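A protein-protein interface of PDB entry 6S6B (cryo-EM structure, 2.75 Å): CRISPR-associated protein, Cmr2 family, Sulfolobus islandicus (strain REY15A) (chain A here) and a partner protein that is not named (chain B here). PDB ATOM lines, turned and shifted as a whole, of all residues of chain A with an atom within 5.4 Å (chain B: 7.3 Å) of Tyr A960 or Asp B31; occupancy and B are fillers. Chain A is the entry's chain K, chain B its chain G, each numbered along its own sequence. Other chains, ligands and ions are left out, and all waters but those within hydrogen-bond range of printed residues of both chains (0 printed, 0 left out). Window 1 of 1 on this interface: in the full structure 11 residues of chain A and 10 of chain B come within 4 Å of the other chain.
The backbone carbonyl oxygen (O) of Tyr A960 is in hydrogen-bond range of the guanidinium group (NH2) of Arg B210 (2.9 Å). The side-chain carboxylate of Asp B31 lies within hydrogen-bond range of the side-chain hydroxyl of Tyr A960 (2.5 Å). The guanidinium group (NH2) of Arg B210 lies within salt-bridge range of the side-chain carboxylate (OD1) of Asp A961 (3.0 Å). The backbone carbonyl oxygen (O) of Glu B27 sits at hydrogen-bond distance from the guanidinium group (NH1) of Arg A1030 (3.0 Å). The guanidinium group (NH1) of Arg A1030 lies within salt-bridge range of the side-chain carboxylate (OE1) of Glu B29, at 3.8 Å. The side-chain carboxylate (OE1) of Glu B29 sits close to the backbone carbonyl oxygen (O) of Leu A959 (3.0 Å). The side-chain carboxylate of Asp B31 lies within salt-bridge range of the guanidinium group of Arg A1030 (3.5 Å).
NE1 of Trp B227 lies within hydrogen-bond range of OE2 of Glu B229, 2.4 Å away. The backbone NH (N) of Asp B31 is in hydrogen-bond range of the backbone carbonyl oxygen (O) of Ser B228, 3.1 Å away.
Among the printed residues, merely in contact across the chains: Ser A957 with Leu B226 (3.5 Å), Arg A1030 with Ile B30 (3.5 Å), Tyr A960 with Leu B226 (3.6 Å), Tyr A960 with Glu B29 (3.9 Å), Val A956 with Leu B226 (3.9 Å) and Tyr A960 with Trp B227 (3.9 Å).
Printed residues of chain B within 4 Å of Ser A957: Leu B226 (3.5 Å). Printed residues of chain B within 4 Å of Leu A959: Glu B29. Tyr A960 touches just these residues of chain B: Glu B29 (3.9 Å), Asp B31 (2.5 Å), Arg B210 (2.9 Å), Leu B226 (3.6 Å) and Trp B227 (3.9 Å). Ser B24 touches none of the printed residues of chain A. Of the printed residues of chain A, Glu B29 touches Leu A959 (3.0 Å), Tyr A960 (3.9 Å) and Arg A1030 (3.8 Å). Of chain A, only Tyr A960 and Arg A1030 come within 4 Å of Asp B31. Of the printed residues of chain A, Leu B226 touches Val A956 (3.9 Å), Ser A957 (3.5 Å) and Tyr A960 (3.6 Å). Of the printed residues of chain A, Trp B227 touches Tyr A960. The nearest printed residue of chain A that does not touch Asp B31 is Val A956 (7.7 Å). The nearest printed residue of chain A that does not touch Leu B226 is Leu A958 (6.0 Å).
Hydrophobic or aromatic side chains of chain B that line the printed part of chain A: Leu B226. Of the 10 printed residues of chain A, 6 touch a printed residue of chain B. Hydrophobic or aromatic side chains of chain A that line the printed part of chain B: Val A956 and Tyr A960. Among the printed residues, 13 pairs touch across the chains. Among the printed residues, Asp or Glu carboxylates within 4 Å of a Lys or Arg side-chain nitrogen of the other chain: Asp A961 with Arg B210, Arg A1030 with Glu B29 and Arg A1030 with Asp B31.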
ATOM      1  N   VAL A 956      13.088 -24.774  -0.581  1.00  0.00           N
ATOM      2  CA  VAL A 956      11.853 -24.430  -1.265  1.00  0.00           C
ATOM      3  C   VAL A 956      10.670 -25.126  -0.618  1.00  0.00           C
ATOM      4  O   VAL A 956       9.519 -24.770  -0.891  1.00  0.00           O
ATOM      5  CB  VAL A 956      11.948 -24.775  -2.763  1.00  0.00           C
ATOM      6  CG1 VAL A 956      11.784 -26.263  -2.979  1.00  0.00           C
ATOM      7  CG2 VAL A 956      10.926 -23.988  -3.554  1.00  0.00           C
ATOM      8  N   SER A 957      10.921 -26.110   0.247  1.00  0.00           N
ATOM      9  CA  SER A 957       9.856 -26.733   1.017  1.00  0.00           C
ATOM     10  C   SER A 957       9.158 -25.751   1.937  1.00  0.00           C
ATOM     11  O   SER A 957       8.097 -26.078   2.475  1.00  0.00           O
ATOM     12  CB  SER A 957      10.414 -27.890   1.834  1.00  0.00           C
ATOM     13  OG  SER A 957      11.116 -27.410   2.961  1.00  0.00           O
ATOM     14  N   LEU A 958       9.740 -24.570   2.142  1.00  0.00           N
ATOM     15  CA  LEU A 958       9.068 -23.510   2.879  1.00  0.00           C
ATOM     16  C   LEU A 958       7.683 -23.248   2.314  1.00  0.00           C
ATOM     17  O   LEU A 958       6.723 -23.031   3.060  1.00  0.00           O
ATOM     18  CB  LEU A 958       9.914 -22.244   2.836  1.00  0.00           C
ATOM     19  CG  LEU A 958       9.360 -21.081   3.642  1.00  0.00           C
ATOM     20  CD1 LEU A 958       9.653 -21.269   5.107  1.00  0.00           C
ATOM     21  CD2 LEU A 958       9.944 -19.791   3.154  1.00  0.00           C
ATOM     22  N   LEU A 959       7.562 -23.266   0.990  1.00  0.00           N
ATOM     23  CA  LEU A 959       6.285 -22.999   0.353  1.00  0.00           C
ATOM     24  C   LEU A 959       5.306 -24.146   0.522  1.00  0.00           C
ATOM     25  O   LEU A 959       4.099 -23.939   0.377  1.00  0.00           O
ATOM     26  CB  LEU A 959       6.497 -22.719  -1.130  1.00  0.00           C
ATOM     27  CG  LEU A 959       7.699 -21.831  -1.429  1.00  0.00           C
ATOM     28  CD1 LEU A 959       7.934 -21.745  -2.919  1.00  0.00           C
ATOM     29  CD2 LEU A 959       7.481 -20.460  -0.844  1.00  0.00           C
ATOM     30  N   TYR A 960       5.792 -25.346   0.816  1.00  0.00           N
ATOM     31  CA  TYR A 960       4.927 -26.510   0.906  1.00  0.00           C
ATOM     32  C   TYR A 960       4.531 -26.855   2.330  1.00  0.00           C
ATOM     33  O   TYR A 960       3.542 -27.569   2.521  1.00  0.00           O
ATOM     34  CB  TYR A 960       5.604 -27.717   0.256  1.00  0.00           C
ATOM     35  CG  TYR A 960       5.921 -27.495  -1.201  1.00  0.00           C
ATOM     36  CD1 TYR A 960       4.963 -27.711  -2.176  1.00  0.00           C
ATOM     37  CD2 TYR A 960       7.169 -27.049  -1.599  1.00  0.00           C
ATOM     38  CE1 TYR A 960       5.243 -27.499  -3.505  1.00  0.00           C
ATOM     39  CE2 TYR A 960       7.458 -26.833  -2.923  1.00  0.00           C
ATOM     40  CZ  TYR A 960       6.492 -27.061  -3.873  1.00  0.00           C
ATOM     41  OH  TYR A 960       6.779 -26.848  -5.200  1.00  0.00           O
ATOM     42  N   ASP A 961       5.263 -26.368   3.326  1.00  0.00           N
ATOM     43  CA  ASP A 961       4.921 -26.633   4.713  1.00  0.00           C
ATOM     44  C   ASP A 961       3.982 -25.601   5.306  1.00  0.00           C
ATOM     45  O   ASP A 961       3.365 -25.874   6.339  1.00  0.00           O
ATOM     46  CB  ASP A 961       6.183 -26.691   5.570  1.00  0.00           C
ATOM     47  CG  ASP A 961       7.169 -27.720   5.078  1.00  0.00           C
ATOM     48  OD1 ASP A 961       6.872 -28.386   4.065  1.00  0.00           O
ATOM     49  OD2 ASP A 961       8.241 -27.865   5.703  1.00  0.00           O
ATOM     50  N   TYR A 962       3.858 -24.428   4.686  1.00  0.00           N
ATOM     51  CA  TYR A 962       3.070 -23.362   5.286  1.00  0.00           C
ATOM     52  C   TYR A 962       1.636 -23.776   5.557  1.00  0.00           C
ATOM     53  O   TYR A 962       0.984 -23.183   6.422  1.00  0.00           O
ATOM     54  CB  TYR A 962       3.062 -22.127   4.396  1.00  0.00           C
ATOM     55  CG  TYR A 962       2.174 -21.046   4.945  1.00  0.00           C
ATOM     56  CD1 TYR A 962       2.526 -20.357   6.092  1.00  0.00           C
ATOM     57  CD2 TYR A 962       0.967 -20.741   4.342  1.00  0.00           C
ATOM     58  CE1 TYR A 962       1.720 -19.382   6.608  1.00  0.00           C
ATOM     59  CE2 TYR A 962       0.152 -19.766   4.853  1.00  0.00           C
ATOM     60  CZ  TYR A 962       0.533 -19.088   5.986  1.00  0.00           C
ATOM     61  OH  TYR A 962      -0.279 -18.107   6.505  1.00  0.00           O
ATOM     62  N   GLU A 963       1.131 -24.781   4.845  1.00  0.00           N
ATOM     63  CA  GLU A 963      -0.268 -25.165   4.989  1.00  0.00           C
ATOM     64  C   GLU A 963      -0.607 -25.528   6.429  1.00  0.00           C
ATOM     65  O   GLU A 963      -1.654 -25.122   6.945  1.00  0.00           O
ATOM     66  CB  GLU A 963      -0.584 -26.319   4.040  1.00  0.00           C
ATOM     67  CG  GLU A 963       0.499 -27.379   3.966  1.00  0.00           C
ATOM     68  CD  GLU A 963       0.354 -28.441   5.030  1.00  0.00           C
ATOM     69  OE1 GLU A 963      -0.756 -28.582   5.582  1.00  0.00           O
ATOM     70  OE2 GLU A 963       1.349 -29.138   5.316  1.00  0.00           O
ATOM     71  N   VAL A1026       3.055 -16.985  -0.260  1.00  0.00           N
ATOM     72  CA  VAL A1026       3.540 -18.299  -0.655  1.00  0.00           C
ATOM     73  C   VAL A1026       3.128 -18.624  -2.080  1.00  0.00           C
ATOM     74  O   VAL A1026       3.920 -19.177  -2.848  1.00  0.00           O
ATOM     75  CB  VAL A1026       3.028 -19.359   0.332  1.00  0.00           C
ATOM     76  CG1 VAL A1026       3.231 -20.747  -0.225  1.00  0.00           C
ATOM     77  CG2 VAL A1026       3.729 -19.210   1.660  1.00  0.00           C
ATOM     78  N   ARG A1030       5.379 -19.471  -5.543  1.00  0.00           N
ATOM     79  CA  ARG A1030       5.152 -20.639  -6.383  1.00  0.00           C
ATOM     80  C   ARG A1030       4.905 -20.234  -7.826  1.00  0.00           C
ATOM     81  O   ARG A1030       5.274 -20.961  -8.753  1.00  0.00           O
ATOM     82  CB  ARG A1030       3.972 -21.445  -5.856  1.00  0.00           C
ATOM     83  CG  ARG A1030       4.245 -22.176  -4.571  1.00  0.00           C
ATOM     84  CD  ARG A1030       3.016 -22.927  -4.133  1.00  0.00           C
ATOM     85  NE  ARG A1030       2.511 -23.786  -5.194  1.00  0.00           N
ATOM     86  CZ  ARG A1030       1.241 -24.150  -5.317  1.00  0.00           C
ATOM     87  NH1 ARG A1030       0.342 -23.727  -4.442  1.00  0.00           N
ATOM     88  NH2 ARG A1030       0.870 -24.936  -6.314  1.00  0.00           N
ATOM     89  N   HIS B  19      -2.886 -40.994 -11.930  1.00  0.00           N
ATOM     90  CA  HIS B  19      -2.579 -39.574 -12.055  1.00  0.00           C
ATOM     91  C   HIS B  19      -2.902 -39.148 -13.479  1.00  0.00           C
ATOM     92  O   HIS B  19      -2.094 -39.344 -14.388  1.00  0.00           O
ATOM     93  CB  HIS B  19      -1.136 -39.257 -11.717  1.00  0.00           C
ATOM     94  CG  HIS B  19      -0.822 -37.802 -11.816  1.00  0.00           C
ATOM     95  ND1 HIS B  19      -0.260 -37.238 -12.938  1.00  0.00           N
ATOM     96  CD2 HIS B  19      -1.027 -36.788 -10.947  1.00  0.00           C
ATOM     97  CE1 HIS B  19      -0.116 -35.940 -12.749  1.00  0.00           C
ATOM     98  NE2 HIS B  19      -0.572 -35.642 -11.547  1.00  0.00           N
ATOM     99  N   SER B  22      -3.515 -32.237 -15.043  1.00  0.00           N
ATOM    100  CA  SER B  22      -4.278 -31.083 -15.490  1.00  0.00           C
ATOM    101  C   SER B  22      -3.441 -29.815 -15.474  1.00  0.00           C
ATOM    102  O   SER B  22      -3.981 -28.713 -15.350  1.00  0.00           O
ATOM    103  CB  SER B  22      -5.516 -30.887 -14.627  1.00  0.00           C
ATOM    104  OG  SER B  22      -5.163 -30.322 -13.379  1.00  0.00           O
ATOM    105  N   GLY B  23      -2.130 -29.942 -15.598  1.00  0.00           N
ATOM    106  CA  GLY B  23      -1.292 -28.762 -15.504  1.00  0.00           C
ATOM    107  C   GLY B  23      -1.191 -28.309 -14.063  1.00  0.00           C
ATOM    108  O   GLY B  23      -0.859 -29.092 -13.169  1.00  0.00           O
ATOM    109  N   SER B  24      -1.486 -27.036 -13.825  1.00  0.00           N
ATOM    110  CA  SER B  24      -1.437 -26.438 -12.497  1.00  0.00           C
ATOM    111  C   SER B  24      -2.713 -25.663 -12.218  1.00  0.00           C
ATOM    112  O   SER B  24      -2.682 -24.513 -11.779  1.00  0.00           O
ATOM    113  CB  SER B  24      -0.214 -25.538 -12.348  1.00  0.00           C
ATOM    114  OG  SER B  24      -0.174 -24.954 -11.062  1.00  0.00           O
ATOM    115  N   SER B  25      -3.861 -26.293 -12.464  1.00  0.00           N
ATOM    116  CA  SER B  25      -5.117 -25.555 -12.527  1.00  0.00           C
ATOM    117  C   SER B  25      -5.663 -25.180 -11.151  1.00  0.00           C
ATOM    118  O   SER B  25      -6.394 -24.191 -11.035  1.00  0.00           O
ATOM    119  CB  SER B  25      -6.151 -26.372 -13.296  1.00  0.00           C
ATOM    120  OG  SER B  25      -6.449 -27.574 -12.609  1.00  0.00           O
ATOM    121  N   VAL B  26      -5.346 -25.940 -10.107  1.00  0.00           N
ATOM    122  CA  VAL B  26      -5.920 -25.710  -8.785  1.00  0.00           C
ATOM    123  C   VAL B  26      -4.814 -25.328  -7.812  1.00  0.00           C
ATOM    124  O   VAL B  26      -3.625 -25.399  -8.139  1.00  0.00           O
ATOM    125  CB  VAL B  26      -6.706 -26.930  -8.266  1.00  0.00           C
ATOM    126  CG1 VAL B  26      -7.845 -27.273  -9.209  1.00  0.00           C
ATOM    127  CG2 VAL B  26      -5.790 -28.105  -8.066  1.00  0.00           C
ATOM    128  N   GLU B  27      -5.221 -24.922  -6.611  1.00  0.00           N
ATOM    129  CA  GLU B  27      -4.356 -24.197  -5.690  1.00  0.00           C
ATOM    130  C   GLU B  27      -3.616 -25.054  -4.673  1.00  0.00           C
ATOM    131  O   GLU B  27      -2.420 -24.845  -4.455  1.00  0.00           O
ATOM    132  CB  GLU B  27      -5.182 -23.159  -4.930  1.00  0.00           C
ATOM    133  CG  GLU B  27      -5.433 -21.873  -5.689  1.00  0.00           C
ATOM    134  CD  GLU B  27      -6.293 -22.073  -6.913  1.00  0.00           C
ATOM    135  OE1 GLU B  27      -6.923 -23.143  -7.038  1.00  0.00           O
ATOM    136  OE2 GLU B  27      -6.344 -21.153  -7.753  1.00  0.00           O
ATOM    137  N   GLU B  28      -4.297 -26.050  -4.101  1.00  0.00           N
ATOM    138  CA  GLU B  28      -4.186 -26.325  -2.670  1.00  0.00           C
ATOM    139  C   GLU B  28      -2.758 -26.198  -2.156  1.00  0.00           C
ATOM    140  O   GLU B  28      -2.437 -25.231  -1.462  1.00  0.00           O
ATOM    141  CB  GLU B  28      -4.705 -27.733  -2.362  1.00  0.00           C
ATOM    142  CG  GLU B  28      -6.218 -27.901  -2.424  1.00  0.00           C
ATOM    143  CD  GLU B  28      -6.759 -27.842  -3.842  1.00  0.00           C
ATOM    144  OE1 GLU B  28      -5.949 -27.874  -4.793  1.00  0.00           O
ATOM    145  OE2 GLU B  28      -7.994 -27.771  -4.005  1.00  0.00           O
ATOM    146  N   GLU B  29      -1.895 -27.145  -2.509  1.00  0.00           N
ATOM    147  CA  GLU B  29      -0.455 -26.929  -2.531  1.00  0.00           C
ATOM    148  C   GLU B  29       0.149 -27.754  -3.652  1.00  0.00           C
ATOM    149  O   GLU B  29       1.366 -27.769  -3.836  1.00  0.00           O
ATOM    150  CB  GLU B  29       0.205 -27.283  -1.194  1.00  0.00           C
ATOM    151  CG  GLU B  29      -0.031 -26.293  -0.058  1.00  0.00           C
ATOM    152  CD  GLU B  29       0.589 -24.922  -0.325  1.00  0.00           C
ATOM    153  OE1 GLU B  29       1.615 -24.849  -1.036  1.00  0.00           O
ATOM    154  OE2 GLU B  29       0.047 -23.917   0.185  1.00  0.00           O
ATOM    155  N   ILE B  30      -0.696 -28.440  -4.400  1.00  0.00           N
ATOM    156  CA  ILE B  30      -0.224 -29.453  -5.329  1.00  0.00           C
ATOM    157  C   ILE B  30       0.231 -28.787  -6.614  1.00  0.00           C
ATOM    158  O   ILE B  30      -0.511 -28.021  -7.233  1.00  0.00           O
ATOM    159  CB  ILE B  30      -1.314 -30.500  -5.602  1.00  0.00           C
ATOM    160  CG1 ILE B  30      -1.745 -31.181  -4.310  1.00  0.00           C
ATOM    161  CG2 ILE B  30      -0.789 -31.555  -6.528  1.00  0.00           C
ATOM    162  CD1 ILE B  30      -2.945 -30.547  -3.661  1.00  0.00           C
ATOM    163  N   ASP B  31       1.463 -29.077  -7.016  1.00  0.00           N
ATOM    164  CA  ASP B  31       2.009 -28.560  -8.260  1.00  0.00           C
ATOM    165  C   ASP B  31       1.444 -29.282  -9.471  1.00  0.00           C
ATOM    166  O   ASP B  31       1.154 -28.649 -10.490  1.00  0.00           O
ATOM    167  CB  ASP B  31       3.531 -28.679  -8.251  1.00  0.00           C
ATOM    168  CG  ASP B  31       4.190 -27.605  -7.422  1.00  0.00           C
ATOM    169  OD1 ASP B  31       3.771 -26.435  -7.520  1.00  0.00           O
ATOM    170  OD2 ASP B  31       5.130 -27.927  -6.669  1.00  0.00           O
ATOM    171  N   LEU B  32       1.285 -30.600  -9.379  1.00  0.00           N
ATOM    172  CA  LEU B  32       0.748 -31.430 -10.453  1.00  0.00           C
ATOM    173  C   LEU B  32      -0.524 -32.091  -9.943  1.00  0.00           C
ATOM    174  O   LEU B  32      -0.505 -33.257  -9.530  1.00  0.00           O
ATOM    175  CB  LEU B  32       1.756 -32.479 -10.912  1.00  0.00           C
ATOM    176  CG  LEU B  32       2.838 -32.067 -11.902  1.00  0.00           C
ATOM    177  CD1 LEU B  32       3.853 -31.154 -11.265  1.00  0.00           C
ATOM    178  CD2 LEU B  32       3.514 -33.301 -12.445  1.00  0.00           C
ATOM    179  N   PRO B  33      -1.642 -31.380  -9.951  1.00  0.00           N
ATOM    180  CA  PRO B  33      -2.878 -31.942  -9.412  1.00  0.00           C
ATOM    181  C   PRO B  33      -3.597 -32.831 -10.411  1.00  0.00           C
ATOM    182  O   PRO B  33      -3.321 -32.832 -11.610  1.00  0.00           O
ATOM    183  CB  PRO B  33      -3.707 -30.699  -9.095  1.00  0.00           C
ATOM    184  CG  PRO B  33      -3.256 -29.715 -10.082  1.00  0.00           C
ATOM    185  CD  PRO B  33      -1.801 -29.966 -10.316  1.00  0.00           C
ATOM    186  N   VAL B 209       1.582 -36.397  -2.454  1.00  0.00           N
ATOM    187  CA  VAL B 209       2.953 -36.695  -2.073  1.00  0.00           C
ATOM    188  C   VAL B 209       3.855 -35.557  -2.511  1.00  0.00           C
ATOM    189  O   VAL B 209       3.543 -34.809  -3.441  1.00  0.00           O
ATOM    190  CB  VAL B 209       3.434 -38.023  -2.684  1.00  0.00           C
ATOM    191  CG1 VAL B 209       2.471 -39.124  -2.358  1.00  0.00           C
ATOM    192  CG2 VAL B 209       3.565 -37.885  -4.173  1.00  0.00           C
ATOM    193  N   ARG B 210       4.972 -35.418  -1.815  1.00  0.00           N
ATOM    194  CA  ARG B 210       6.091 -34.635  -2.304  1.00  0.00           C
ATOM    195  C   ARG B 210       7.054 -35.564  -3.019  1.00  0.00           C
ATOM    196  O   ARG B 210       7.150 -36.750  -2.700  1.00  0.00           O
ATOM    197  CB  ARG B 210       6.814 -33.925  -1.166  1.00  0.00           C
ATOM    198  CG  ARG B 210       6.032 -32.840  -0.476  1.00  0.00           C
ATOM    199  CD  ARG B 210       6.847 -32.291   0.677  1.00  0.00           C
ATOM    200  NE  ARG B 210       6.214 -31.154   1.328  1.00  0.00           N
ATOM    201  CZ  ARG B 210       5.316 -31.261   2.299  1.00  0.00           C
ATOM    202  NH1 ARG B 210       4.944 -32.457   2.730  1.00  0.00           N
ATOM    203  NH2 ARG B 210       4.787 -30.174   2.839  1.00  0.00           N
ATOM    204  N   GLY B 224      15.373 -26.399  -5.736  1.00  0.00           N
ATOM    205  CA  GLY B 224      14.102 -26.464  -6.431  1.00  0.00           C
ATOM    206  C   GLY B 224      13.815 -27.823  -7.022  1.00  0.00           C
ATOM    207  O   GLY B 224      13.068 -27.923  -8.001  1.00  0.00           O
ATOM    208  N   LEU B 226      12.219 -30.098  -5.516  1.00  0.00           N
ATOM    209  CA  LEU B 226      11.083 -30.583  -4.750  1.00  0.00           C
ATOM    210  C   LEU B 226       9.800 -30.078  -5.387  1.00  0.00           C
ATOM    211  O   LEU B 226       9.684 -28.888  -5.691  1.00  0.00           O
ATOM    212  CB  LEU B 226      11.164 -30.122  -3.298  1.00  0.00           C
ATOM    213  CG  LEU B 226       9.901 -30.315  -2.465  1.00  0.00           C
ATOM    214  CD1 LEU B 226       9.681 -31.755  -2.101  1.00  0.00           C
ATOM    215  CD2 LEU B 226       9.987 -29.487  -1.236  1.00  0.00           C
ATOM    216  N   TRP B 227       8.846 -30.978  -5.590  1.00  0.00           N
ATOM    217  CA  TRP B 227       7.540 -30.607  -6.106  1.00  0.00           C
ATOM    218  C   TRP B 227       6.511 -31.557  -5.514  1.00  0.00           C
ATOM    219  O   TRP B 227       6.847 -32.503  -4.802  1.00  0.00           O
ATOM    220  CB  TRP B 227       7.526 -30.618  -7.635  1.00  0.00           C
ATOM    221  CG  TRP B 227       7.392 -31.964  -8.212  1.00  0.00           C
ATOM    222  CD1 TRP B 227       6.255 -32.554  -8.645  1.00  0.00           C
ATOM    223  CD2 TRP B 227       8.441 -32.903  -8.427  1.00  0.00           C
ATOM    224  NE1 TRP B 227       6.524 -33.809  -9.117  1.00  0.00           N
ATOM    225  CE2 TRP B 227       7.864 -34.047  -8.990  1.00  0.00           C
ATOM    226  CE3 TRP B 227       9.814 -32.887  -8.194  1.00  0.00           C
ATOM    227  CZ2 TRP B 227       8.608 -35.161  -9.326  1.00  0.00           C
ATOM    228  CZ3 TRP B 227      10.546 -33.990  -8.523  1.00  0.00           C
ATOM    229  CH2 TRP B 227       9.946 -35.115  -9.077  1.00  0.00           C
ATOM    230  N   SER B 228       5.245 -31.302  -5.816  1.00  0.00           N
ATOM    231  CA  SER B 228       4.143 -32.010  -5.190  1.00  0.00           C
ATOM    232  C   SER B 228       3.179 -32.513  -6.251  1.00  0.00           C
ATOM    233  O   SER B 228       2.939 -31.836  -7.251  1.00  0.00           O
ATOM    234  CB  SER B 228       3.413 -31.104  -4.207  1.00  0.00           C
ATOM    235  OG  SER B 228       2.333 -31.779  -3.599  1.00  0.00           O
ATOM    236  N   GLU B 229       2.630 -33.702  -6.026  1.00  0.00           N
ATOM    237  CA  GLU B 229       1.706 -34.325  -6.959  1.00  0.00           C
ATOM    238  C   GLU B 229       0.536 -34.904  -6.189  1.00  0.00           C
ATOM    239  O   GLU B 229       0.571 -35.029  -4.965  1.00  0.00           O
ATOM    240  CB  GLU B 229       2.374 -35.430  -7.766  1.00  0.00           C
ATOM    241  CG  GLU B 229       3.475 -34.949  -8.649  1.00  0.00           C
ATOM    242  CD  GLU B 229       4.287 -36.079  -9.207  1.00  0.00           C
ATOM    243  OE1 GLU B 229       3.900 -37.245  -8.992  1.00  0.00           O
ATOM    244  OE2 GLU B 229       5.312 -35.803  -9.861  1.00  0.00           O
ATOM    245  N   GLU B 230      -0.502 -35.279  -6.925  1.00  0.00           N
ATOM    246  CA  GLU B 230      -1.716 -35.819  -6.338  1.00  0.00           C
ATOM    247  C   GLU B 230      -2.119 -37.073  -7.089  1.00  0.00           C
ATOM    248  O   GLU B 230      -2.208 -37.060  -8.316  1.00  0.00           O
ATOM    249  CB  GLU B 230      -2.849 -34.801  -6.383  1.00  0.00           C
ATOM    250  CG  GLU B 230      -4.181 -35.374  -5.970  1.00  0.00           C
ATOM    251  CD  GLU B 230      -5.317 -34.402  -6.182  1.00  0.00           C
ATOM    252  OE1 GLU B 230      -5.114 -33.192  -5.951  1.00  0.00           O
ATOM    253  OE2 GLU B 230      -6.412 -34.845  -6.585  1.00  0.00           O
